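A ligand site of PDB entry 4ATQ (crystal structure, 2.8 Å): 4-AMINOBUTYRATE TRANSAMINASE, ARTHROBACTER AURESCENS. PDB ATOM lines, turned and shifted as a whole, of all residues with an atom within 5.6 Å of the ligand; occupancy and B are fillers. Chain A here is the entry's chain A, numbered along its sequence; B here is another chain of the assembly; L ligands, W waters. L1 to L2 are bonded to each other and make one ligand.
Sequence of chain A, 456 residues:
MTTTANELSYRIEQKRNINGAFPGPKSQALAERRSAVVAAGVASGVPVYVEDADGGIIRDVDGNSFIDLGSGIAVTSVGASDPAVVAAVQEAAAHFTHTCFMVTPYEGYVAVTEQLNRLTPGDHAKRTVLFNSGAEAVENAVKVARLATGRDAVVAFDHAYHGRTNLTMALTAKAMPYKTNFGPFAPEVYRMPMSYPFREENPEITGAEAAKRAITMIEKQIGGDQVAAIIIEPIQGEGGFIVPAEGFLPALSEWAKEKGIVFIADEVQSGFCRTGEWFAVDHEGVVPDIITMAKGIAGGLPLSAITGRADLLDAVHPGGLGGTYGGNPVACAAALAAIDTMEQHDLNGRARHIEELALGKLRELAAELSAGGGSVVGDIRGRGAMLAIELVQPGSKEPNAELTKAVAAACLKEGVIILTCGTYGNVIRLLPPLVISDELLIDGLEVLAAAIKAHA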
ATOM      1  N   ILE A  73       7.524 -13.679  35.024  1.00  0.00           N
ATOM      2  CA  ILE A  73       6.795 -12.454  35.223  1.00  0.00           C
ATOM      3  C   ILE A  73       5.357 -12.762  35.584  1.00  0.00           C
ATOM      4  O   ILE A  73       4.411 -12.437  34.850  1.00  0.00           O
ATOM      5  CB  ILE A  73       6.867 -11.455  34.050  1.00  0.00           C
ATOM      6  CG1 ILE A  73       8.212 -11.507  33.338  1.00  0.00           C
ATOM      7  CG2 ILE A  73       6.641 -10.052  34.567  1.00  0.00           C
ATOM      8  CD1 ILE A  73       8.480 -10.347  32.403  1.00  0.00           C
ATOM      9  N   SER A 133      -2.866 -12.396  24.233  1.00  0.00           N
ATOM     10  CA  SER A 133      -1.952 -11.630  25.094  1.00  0.00           C
ATOM     11  C   SER A 133      -2.654 -10.653  25.990  1.00  0.00           C
ATOM     12  O   SER A 133      -3.778 -10.244  25.728  1.00  0.00           O
ATOM     13  CB  SER A 133      -0.969 -10.835  24.233  1.00  0.00           C
ATOM     14  OG  SER A 133      -1.636  -9.852  23.450  1.00  0.00           O
ATOM     15  N   GLY A 134      -1.967 -10.197  27.002  1.00  0.00           N
ATOM     16  CA  GLY A 134      -2.494  -9.121  27.850  1.00  0.00           C
ATOM     17  C   GLY A 134      -2.776  -7.859  27.043  1.00  0.00           C
ATOM     18  O   GLY A 134      -3.794  -7.222  27.215  1.00  0.00           O
ATOM     19  N   ALA A 135      -1.824  -7.482  26.181  1.00  0.00           N
ATOM     20  CA  ALA A 135      -2.002  -6.332  25.301  1.00  0.00           C
ATOM     21  C   ALA A 135      -3.315  -6.443  24.491  1.00  0.00           C
ATOM     22  O   ALA A 135      -4.067  -5.506  24.427  1.00  0.00           O
ATOM     23  CB  ALA A 135      -0.824  -6.201  24.327  1.00  0.00           C
ATOM     24  N   GLU A 136      -3.591  -7.622  23.975  1.00  0.00           N
ATOM     25  CA  GLU A 136      -4.809  -7.780  23.231  1.00  0.00           C
ATOM     26  C   GLU A 136      -6.006  -7.553  24.146  1.00  0.00           C
ATOM     27  O   GLU A 136      -7.001  -6.954  23.746  1.00  0.00           O
ATOM     28  CB  GLU A 136      -4.845  -9.181  22.560  1.00  0.00           C
ATOM     29  CG  GLU A 136      -4.041  -9.246  21.266  1.00  0.00           C
ATOM     30  CD  GLU A 136      -4.128 -10.583  20.579  1.00  0.00           C
ATOM     31  OE1 GLU A 136      -4.128 -11.636  21.308  1.00  0.00           O
ATOM     32  OE2 GLU A 136      -4.284 -10.586  19.300  1.00  0.00           O
ATOM     33  N   VAL A 138      -6.237  -5.684  26.892  1.00  0.00           N
ATOM     34  CA  VAL A 138      -6.408  -4.238  27.131  1.00  0.00           C
ATOM     35  C   VAL A 138      -6.947  -3.540  25.865  1.00  0.00           C
ATOM     36  O   VAL A 138      -7.856  -2.709  25.942  1.00  0.00           O
ATOM     37  CB  VAL A 138      -5.086  -3.572  27.603  1.00  0.00           C
ATOM     38  CG1 VAL A 138      -5.237  -2.053  27.640  1.00  0.00           C
ATOM     39  CG2 VAL A 138      -4.660  -4.141  28.971  1.00  0.00           C
ATOM     40  N   TYR A 161       1.663   0.549  33.168  1.00  0.00           N
ATOM     41  CA  TYR A 161       2.161  -0.299  32.077  1.00  0.00           C
ATOM     42  C   TYR A 161       1.000  -1.175  31.599  1.00  0.00           C
ATOM     43  O   TYR A 161       0.372  -1.824  32.407  1.00  0.00           O
ATOM     44  CB  TYR A 161       3.338  -1.174  32.495  1.00  0.00           C
ATOM     45  CG  TYR A 161       3.806  -2.021  31.348  1.00  0.00           C
ATOM     46  CD1 TYR A 161       3.183  -3.231  31.057  1.00  0.00           C
ATOM     47  CD2 TYR A 161       4.787  -1.583  30.489  1.00  0.00           C
ATOM     48  CE1 TYR A 161       3.557  -3.962  29.947  1.00  0.00           C
ATOM     49  CE2 TYR A 161       5.160  -2.327  29.394  1.00  0.00           C
ATOM     50  CZ  TYR A 161       4.551  -3.503  29.123  1.00  0.00           C
ATOM     51  OH  TYR A 161       4.951  -4.264  28.057  1.00  0.00           O
ATOM     52  N   HIS A 162       0.733  -1.177  30.292  1.00  0.00           N
ATOM     53  CA  HIS A 162      -0.381  -1.935  29.737  1.00  0.00           C
ATOM     54  C   HIS A 162      -0.070  -2.679  28.459  1.00  0.00           C
ATOM     55  O   HIS A 162      -0.941  -3.364  27.919  1.00  0.00           O
ATOM     56  CB  HIS A 162      -1.570  -1.007  29.487  1.00  0.00           C
ATOM     57  CG  HIS A 162      -2.080  -0.314  30.734  1.00  0.00           C
ATOM     58  ND1 HIS A 162      -2.797  -0.950  31.677  1.00  0.00           N
ATOM     59  CD2 HIS A 162      -1.973   1.029  31.159  1.00  0.00           C
ATOM     60  CE1 HIS A 162      -3.100  -0.078  32.666  1.00  0.00           C
ATOM     61  NE2 HIS A 162      -2.610   1.137  32.349  1.00  0.00           N
ATOM     62  N   GLY A 163       1.138  -2.560  27.924  1.00  0.00           N
ATOM     63  CA  GLY A 163       1.500  -3.370  26.755  1.00  0.00           C
ATOM     64  C   GLY A 163       2.353  -2.702  25.696  1.00  0.00           C
ATOM     65  O   GLY A 163       2.678  -1.522  25.786  1.00  0.00           O
ATOM     66  N   ARG A 164       2.640  -3.473  24.660  1.00  0.00           N
ATOM     67  CA  ARG A 164       3.583  -3.089  23.627  1.00  0.00           C
ATOM     68  C   ARG A 164       2.997  -2.914  22.209  1.00  0.00           C
ATOM     69  O   ARG A 164       3.746  -2.683  21.256  1.00  0.00           O
ATOM     70  CB  ARG A 164       4.691  -4.142  23.566  1.00  0.00           C
ATOM     71  CG  ARG A 164       5.569  -4.182  24.804  1.00  0.00           C
ATOM     72  CD  ARG A 164       6.606  -5.237  24.623  1.00  0.00           C
ATOM     73  NE  ARG A 164       7.516  -5.330  25.765  1.00  0.00           N
ATOM     74  CZ  ARG A 164       8.753  -4.821  25.842  1.00  0.00           C
ATOM     75  NH1 ARG A 164       9.279  -4.109  24.848  1.00  0.00           N
ATOM     76  NH2 ARG A 164       9.449  -4.998  26.962  1.00  0.00           N
ATOM     77  N   TYR A 178       9.972   0.783  26.326  1.00  0.00           N
ATOM     78  CA  TYR A 178       8.705   0.360  25.714  1.00  0.00           C
ATOM     79  C   TYR A 178       8.215   1.248  24.545  1.00  0.00           C
ATOM     80  O   TYR A 178       7.435   0.773  23.733  1.00  0.00           O
ATOM     81  CB  TYR A 178       7.624   0.269  26.777  1.00  0.00           C
ATOM     82  CG  TYR A 178       8.045  -0.405  28.036  1.00  0.00           C
ATOM     83  CD1 TYR A 178       8.371  -1.761  28.047  1.00  0.00           C
ATOM     84  CD2 TYR A 178       8.090   0.290  29.235  1.00  0.00           C
ATOM     85  CE1 TYR A 178       8.757  -2.398  29.226  1.00  0.00           C
ATOM     86  CE2 TYR A 178       8.478  -0.332  30.414  1.00  0.00           C
ATOM     87  CZ  TYR A 178       8.807  -1.669  30.402  1.00  0.00           C
ATOM     88  OH  TYR A 178       9.190  -2.255  31.587  1.00  0.00           O
ATOM     89  N   GLU A 233      -4.149  -0.232  36.974  1.00  0.00           N
ATOM     90  CA  GLU A 233      -3.702  -1.470  37.593  1.00  0.00           C
ATOM     91  C   GLU A 233      -3.902  -1.283  39.087  1.00  0.00           C
ATOM     92  O   GLU A 233      -3.366  -0.327  39.639  1.00  0.00           O
ATOM     93  CB  GLU A 233      -2.212  -1.709  37.327  1.00  0.00           C
ATOM     94  CG  GLU A 233      -1.805  -1.796  35.869  1.00  0.00           C
ATOM     95  CD  GLU A 233      -0.312  -1.601  35.696  1.00  0.00           C
ATOM     96  OE1 GLU A 233       0.439  -2.555  36.001  1.00  0.00           O
ATOM     97  OE2 GLU A 233       0.085  -0.474  35.342  1.00  0.00           O
ATOM     98  N   GLY A 237       2.351  -2.864  38.226  1.00  0.00           N
ATOM     99  CA  GLY A 237       3.432  -3.835  38.140  1.00  0.00           C
ATOM    100  C   GLY A 237       4.750  -3.247  37.731  1.00  0.00           C
ATOM    101  O   GLY A 237       5.578  -2.855  38.582  1.00  0.00           O
ATOM    102  N   GLU A 238       4.991  -3.159  36.436  1.00  0.00           N
ATOM    103  CA  GLU A 238       6.258  -2.639  35.932  1.00  0.00           C
ATOM    104  C   GLU A 238       6.581  -1.277  36.523  1.00  0.00           C
ATOM    105  O   GLU A 238       7.730  -0.892  36.586  1.00  0.00           O
ATOM    106  CB  GLU A 238       6.265  -2.555  34.427  1.00  0.00           C
ATOM    107  CG  GLU A 238       5.881  -3.848  33.741  1.00  0.00           C
ATOM    108  CD  GLU A 238       6.718  -5.038  34.170  1.00  0.00           C
ATOM    109  OE1 GLU A 238       7.956  -4.937  34.082  1.00  0.00           O
ATOM    110  OE2 GLU A 238       6.132  -6.080  34.522  1.00  0.00           O
ATOM    111  N   ASP A 266      -6.892  -3.315  35.170  1.00  0.00           N
ATOM    112  CA  ASP A 266      -5.948  -4.166  34.500  1.00  0.00           C
ATOM    113  C   ASP A 266      -5.320  -5.141  35.487  1.00  0.00           C
ATOM    114  O   ASP A 266      -4.387  -4.794  36.176  1.00  0.00           O
ATOM    115  CB  ASP A 266      -4.880  -3.346  33.820  1.00  0.00           C
ATOM    116  CG  ASP A 266      -3.986  -4.185  32.937  1.00  0.00           C
ATOM    117  OD1 ASP A 266      -4.179  -5.431  32.926  1.00  0.00           O
ATOM    118  OD2 ASP A 266      -3.153  -3.590  32.228  1.00  0.00           O
ATOM    119  N   VAL A 268      -3.881  -8.058  34.709  1.00  0.00           N
ATOM    120  CA  VAL A 268      -3.078  -8.971  33.951  1.00  0.00           C
ATOM    121  C   VAL A 268      -1.960  -9.572  34.824  1.00  0.00           C
ATOM    122  O   VAL A 268      -1.764 -10.782  34.815  1.00  0.00           O
ATOM    123  CB  VAL A 268      -2.497  -8.288  32.667  1.00  0.00           C
ATOM    124  CG1 VAL A 268      -1.280  -9.005  32.164  1.00  0.00           C
ATOM    125  CG2 VAL A 268      -3.536  -8.251  31.593  1.00  0.00           C
ATOM    126  N   GLN A 269      -1.257  -8.723  35.570  1.00  0.00           N
ATOM    127  CA  GLN A 269      -0.186  -9.160  36.450  1.00  0.00           C
ATOM    128  C   GLN A 269      -0.710  -9.523  37.867  1.00  0.00           C
ATOM    129  O   GLN A 269      -0.257 -10.514  38.440  1.00  0.00           O
ATOM    130  CB  GLN A 269       0.918  -8.115  36.546  1.00  0.00           C
ATOM    131  CG  GLN A 269       2.205  -8.656  37.117  1.00  0.00           C
ATOM    132  CD  GLN A 269       3.396  -7.700  36.968  1.00  0.00           C
ATOM    133  OE1 GLN A 269       3.491  -6.959  35.998  1.00  0.00           O
ATOM    134  NE2 GLN A 269       4.313  -7.738  37.931  1.00  0.00           N
ATOM    135  N   ALA A 294      -4.628 -11.976  31.898  1.00  0.00           N
ATOM    136  CA  ALA A 294      -3.742 -12.880  31.131  1.00  0.00           C
ATOM    137  C   ALA A 294      -2.816 -13.619  32.112  1.00  0.00           C
ATOM    138  O   ALA A 294      -3.268 -14.032  33.169  1.00  0.00           O
ATOM    139  CB  ALA A 294      -2.939 -12.133  30.069  1.00  0.00           C
ATOM    140  N   LYS A 295      -1.552 -13.808  31.740  1.00  0.00           N
ATOM    141  CA  LYS A 295      -0.512 -14.385  32.598  1.00  0.00           C
ATOM    142  C   LYS A 295      -0.959 -15.657  33.342  1.00  0.00           C
ATOM    143  O   LYS A 295      -0.979 -16.747  32.777  1.00  0.00           O
ATOM    144  CB  LYS A 295       0.016 -13.293  33.540  1.00  0.00           C
ATOM    145  CG  LYS A 295       1.025 -12.327  32.918  1.00  0.00           C
ATOM    146  CD  LYS A 295       1.239 -11.093  33.786  1.00  0.00           C
ATOM    147  CE  LYS A 295       2.549 -10.292  33.594  1.00  0.00           C
ATOM    148  NZ  LYS A 295       3.148 -10.173  32.251  1.00  0.00           N
ATOM    149  N   MET B 102      12.337 -13.426  27.438  1.00  0.00           N
ATOM    150  CA  MET B 102      13.022 -12.215  27.941  1.00  0.00           C
ATOM    151  C   MET B 102      13.616 -12.399  29.352  1.00  0.00           C
ATOM    152  O   MET B 102      14.460 -11.616  29.746  1.00  0.00           O
ATOM    153  CB  MET B 102      12.075 -11.026  28.051  1.00  0.00           C
ATOM    154  CG  MET B 102      11.511 -10.433  26.769  1.00  0.00           C
ATOM    155  SD  MET B 102      10.149  -9.323  27.241  1.00  0.00           S
ATOM    156  CE  MET B 102      10.927  -8.392  28.584  1.00  0.00           C
ATOM    157  N   GLU B 136      -0.025  -8.910  16.559  1.00  0.00           N
ATOM    158  CA  GLU B 136       1.176  -8.529  17.286  1.00  0.00           C
ATOM    159  C   GLU B 136       2.361  -8.486  16.288  1.00  0.00           C
ATOM    160  O   GLU B 136       3.219  -7.599  16.372  1.00  0.00           O
ATOM    161  CB  GLU B 136       1.454  -9.486  18.461  1.00  0.00           C
ATOM    162  CG  GLU B 136       0.676  -9.163  19.692  1.00  0.00           C
ATOM    163  CD  GLU B 136       0.998 -10.098  20.851  1.00  0.00           C
ATOM    164  OE1 GLU B 136       1.131 -11.317  20.609  1.00  0.00           O
ATOM    165  OE2 GLU B 136       1.078  -9.582  22.016  1.00  0.00           O
ATOM    166  N   GLY B 322       9.022  -7.111  22.492  1.00  0.00           N
ATOM    167  CA  GLY B 322       8.751  -8.291  23.314  1.00  0.00           C
ATOM    168  C   GLY B 322       7.301  -8.467  23.712  1.00  0.00           C
ATOM    169  O   GLY B 322       6.386  -8.212  22.945  1.00  0.00           O
ATOM    170  N   GLY B 323       7.122  -8.961  24.947  1.00  0.00           N
ATOM    171  CA  GLY B 323       5.830  -9.507  25.411  1.00  0.00           C
ATOM    172  C   GLY B 323       6.039 -10.657  26.390  1.00  0.00           C
ATOM    173  O   GLY B 323       7.150 -11.149  26.550  1.00  0.00           O
ATOM    174  N   THR B 324       4.989 -11.079  27.064  1.00  0.00           N
ATOM    175  CA  THR B 324       5.124 -12.108  28.088  1.00  0.00           C
ATOM    176  C   THR B 324       5.161 -13.495  27.480  1.00  0.00           C
ATOM    177  O   THR B 324       6.173 -14.177  27.551  1.00  0.00           O
ATOM    178  CB  THR B 324       4.002 -11.994  29.128  1.00  0.00           C
ATOM    179  OG1 THR B 324       4.055 -10.685  29.731  1.00  0.00           O
ATOM    180  CG2 THR B 324       4.089 -13.144  30.171  1.00  0.00           C
ATOM    181  N   TYR B 325       4.071 -13.882  26.829  1.00  0.00           N
ATOM    182  CA  TYR B 325       3.903 -15.215  26.270  1.00  0.00           C
ATOM    183  C   TYR B 325       4.767 -15.501  25.043  1.00  0.00           C
ATOM    184  O   TYR B 325       5.033 -16.643  24.725  1.00  0.00           O
ATOM    185  CB  TYR B 325       2.448 -15.409  25.827  1.00  0.00           C
ATOM    186  CG  TYR B 325       1.384 -15.523  26.912  1.00  0.00           C
ATOM    187  CD1 TYR B 325       1.555 -16.310  28.037  1.00  0.00           C
ATOM    188  CD2 TYR B 325       0.139 -14.912  26.748  1.00  0.00           C
ATOM    189  CE1 TYR B 325       0.547 -16.453  28.967  1.00  0.00           C
ATOM    190  CE2 TYR B 325      -0.877 -15.040  27.677  1.00  0.00           C
ATOM    191  CZ  TYR B 325      -0.664 -15.819  28.787  1.00  0.00           C
ATOM    192  OH  TYR B 325      -1.683 -15.962  29.703  1.00  0.00           O
HETATM  193  N1  LIG L   1      -1.012  -5.177  31.657  1.00  0.00           N
HETATM  194  C1  LIG L   1      -0.152  -5.332  32.682  1.00  0.00           C
HETATM  195  C2  LIG L   1      -0.453  -4.797  33.963  1.00  0.00           C
HETATM  196  C3  LIG L   1       1.064  -5.994  32.446  1.00  0.00           C
HETATM  197  O1  LIG L   1       1.905  -6.072  33.538  1.00  0.00           O
HETATM  198  C4  LIG L   1       1.458  -6.513  31.206  1.00  0.00           C
HETATM  199  C5  LIG L   1       2.691  -7.198  30.977  1.00  0.00           C
HETATM  200  C6  LIG L   1       0.547  -6.363  30.196  1.00  0.00           C
HETATM  201  C7  LIG L   1      -0.669  -5.701  30.432  1.00  0.00           C
HETATM  202  C8  LIG L   1       0.781  -6.802  28.926  1.00  0.00           C
HETATM  203  O2  LIG L   1       0.527  -8.186  28.837  1.00  0.00           O
HETATM  204  P1  LIG L   1       1.207  -9.177  27.694  1.00  0.00           P
HETATM  205  O3  LIG L   1       0.682  -8.660  26.281  1.00  0.00           O
HETATM  206  O4  LIG L   1       2.798  -8.941  27.653  1.00  0.00           O
HETATM  207  O5  LIG L   1       0.839 -10.585  27.947  1.00  0.00           O
HETATM  208  N1  LG2 L   2       3.725  -7.134  31.898  1.00  0.00           N
HETATM  209  C1  LG2 L   2       4.995  -7.838  31.833  1.00  0.00           C
HETATM  210  C2  LG2 L   2       6.032  -6.954  31.059  1.00  0.00           C
HETATM  211  C3  LG2 L   2       6.436  -7.753  29.811  1.00  0.00           C
HETATM  212  C4  LG2 L   2       7.303  -6.989  28.853  1.00  0.00           C
HETATM  213  O1  LG2 L   2       8.093  -6.166  29.331  1.00  0.00           O
HETATM  214  O2  LG2 L   2       7.185  -7.288  27.637  1.00  0.00           O
HETATM  215  O   HOH W   1       4.286  -6.788  27.403  1.00  0.00           O
HETATM  216  O   HOH W   2       2.658  -3.728  34.745  1.00  0.00           O
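The side-chain carboxylate (OD2) of Asp 266 lies within hydrogen-bond range of a nitrogen (N1) of LIG L1 (2.7 Å). The guanidinium group of Arg 164 lies within salt-bridge range of an oxygen (O2) of LG2 L2 (2.7 Å). N of Ala 135 is in hydrogen-bond range of O3 of LIG L1. An oxygen (O5) of LIG L1 is in hydrogen-bond range of the backbone NH (N) of Gly 134, at 3.0 Å. The backbone NH (N) of Thr 324 of chain B is in hydrogen-bond range of an oxygen (O4) of LIG L1, 3.1 Å away. O4 of LIG L1 sits at hydrogen-bond distance from OG1 of Thr 324 of chain B. NZ of Lys 295 sits close to N1 of LG2 L2. OE1 of Gln 269 is in hydrogen-bond range of O1 of LIG L1. The backbone NH of Gly 323 of chain B is in hydrogen-bond range of an oxygen (O2) of LG2 L2.
OD2 of Asp 266 is in hydrogen-bond range of ND1 of His 162 (2.7 Å). N of Val 268 sits close to OD1 of Asp 266 (3.2 Å). The side-chain amino group (NZ) of Lys 295 lies within hydrogen-bond range of the side-chain hydroxyl (OG1) of Thr 324 of chain B (2.7 Å). N of Lys 295 lies within hydrogen-bond range of OH of Tyr 325 of chain B (3.0 Å). The side-chain carboxylate of Glu 238 lies close to the side-chain amide oxygen of Gln 269 (3.2 Å). OE2 of Glu 233 lies within hydrogen-bond range of N of Tyr 161 (2.9 Å). The side-chain carboxylate (OE1) of Glu 233 is in hydrogen-bond range of the backbone NH (N) of Gly 237, 2.9 Å away. The side-chain hydroxyl (OG) of Ser 133 sits at hydrogen-bond distance from the side-chain carboxylate (OE2) of Glu 136 of chain B (3.1 Å).
SD of Met 102 of chain B lies close to O2 of LG2 L2 (3.6 Å). CG2 of Ile 73 touches C1 of LG2 L2, 3.9 Å away. CB of Ser 133 touches O3 of LIG L1, at 3.4 Å. O of Tyr 161 touches C2 of LIG L1, 3.5 Å away. His 162 touches the ligand. CE1 of Tyr 178 touches O1 of LG2 L2 (3.8 Å). OE1 of Glu 233 touches C2 of LIG L1, at 3.2 Å. OE2 of Glu 238 touches C1 of LG2 L2, at 3.4 Å. CB of Val 268 touches N1 of LIG L1, at 3.6 Å. Hydrophobic or aromatic side chains that line the ligand: Ile 73, Ala 135, Tyr 161, Tyr 178, Val 268 and Met 102 of chain B. 17 residues have an atom within 4 Å of the ligand: Ile 73, Ser 133, Gly 134, Ala 135, Tyr 161, His 162, Arg 164, Tyr 178, Glu 233, Glu 238, Asp 266, Val 268, Gln 269, Lys 295, Met 102 of chain B, Gly 323 of chain B and Thr 324 of chain B.
Water W1 bridges an oxygen (O4) of LIG L1 (2.6 Å) and the side-chain hydroxyl (OH) of Tyr 161 (2.7 Å). Water W2 lies within hydrogen-bond range of O1 of LIG L1 (2.7 Å), OE1 of Glu 233 (2.8 Å) and N of Glu 238 (2.9 Å).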
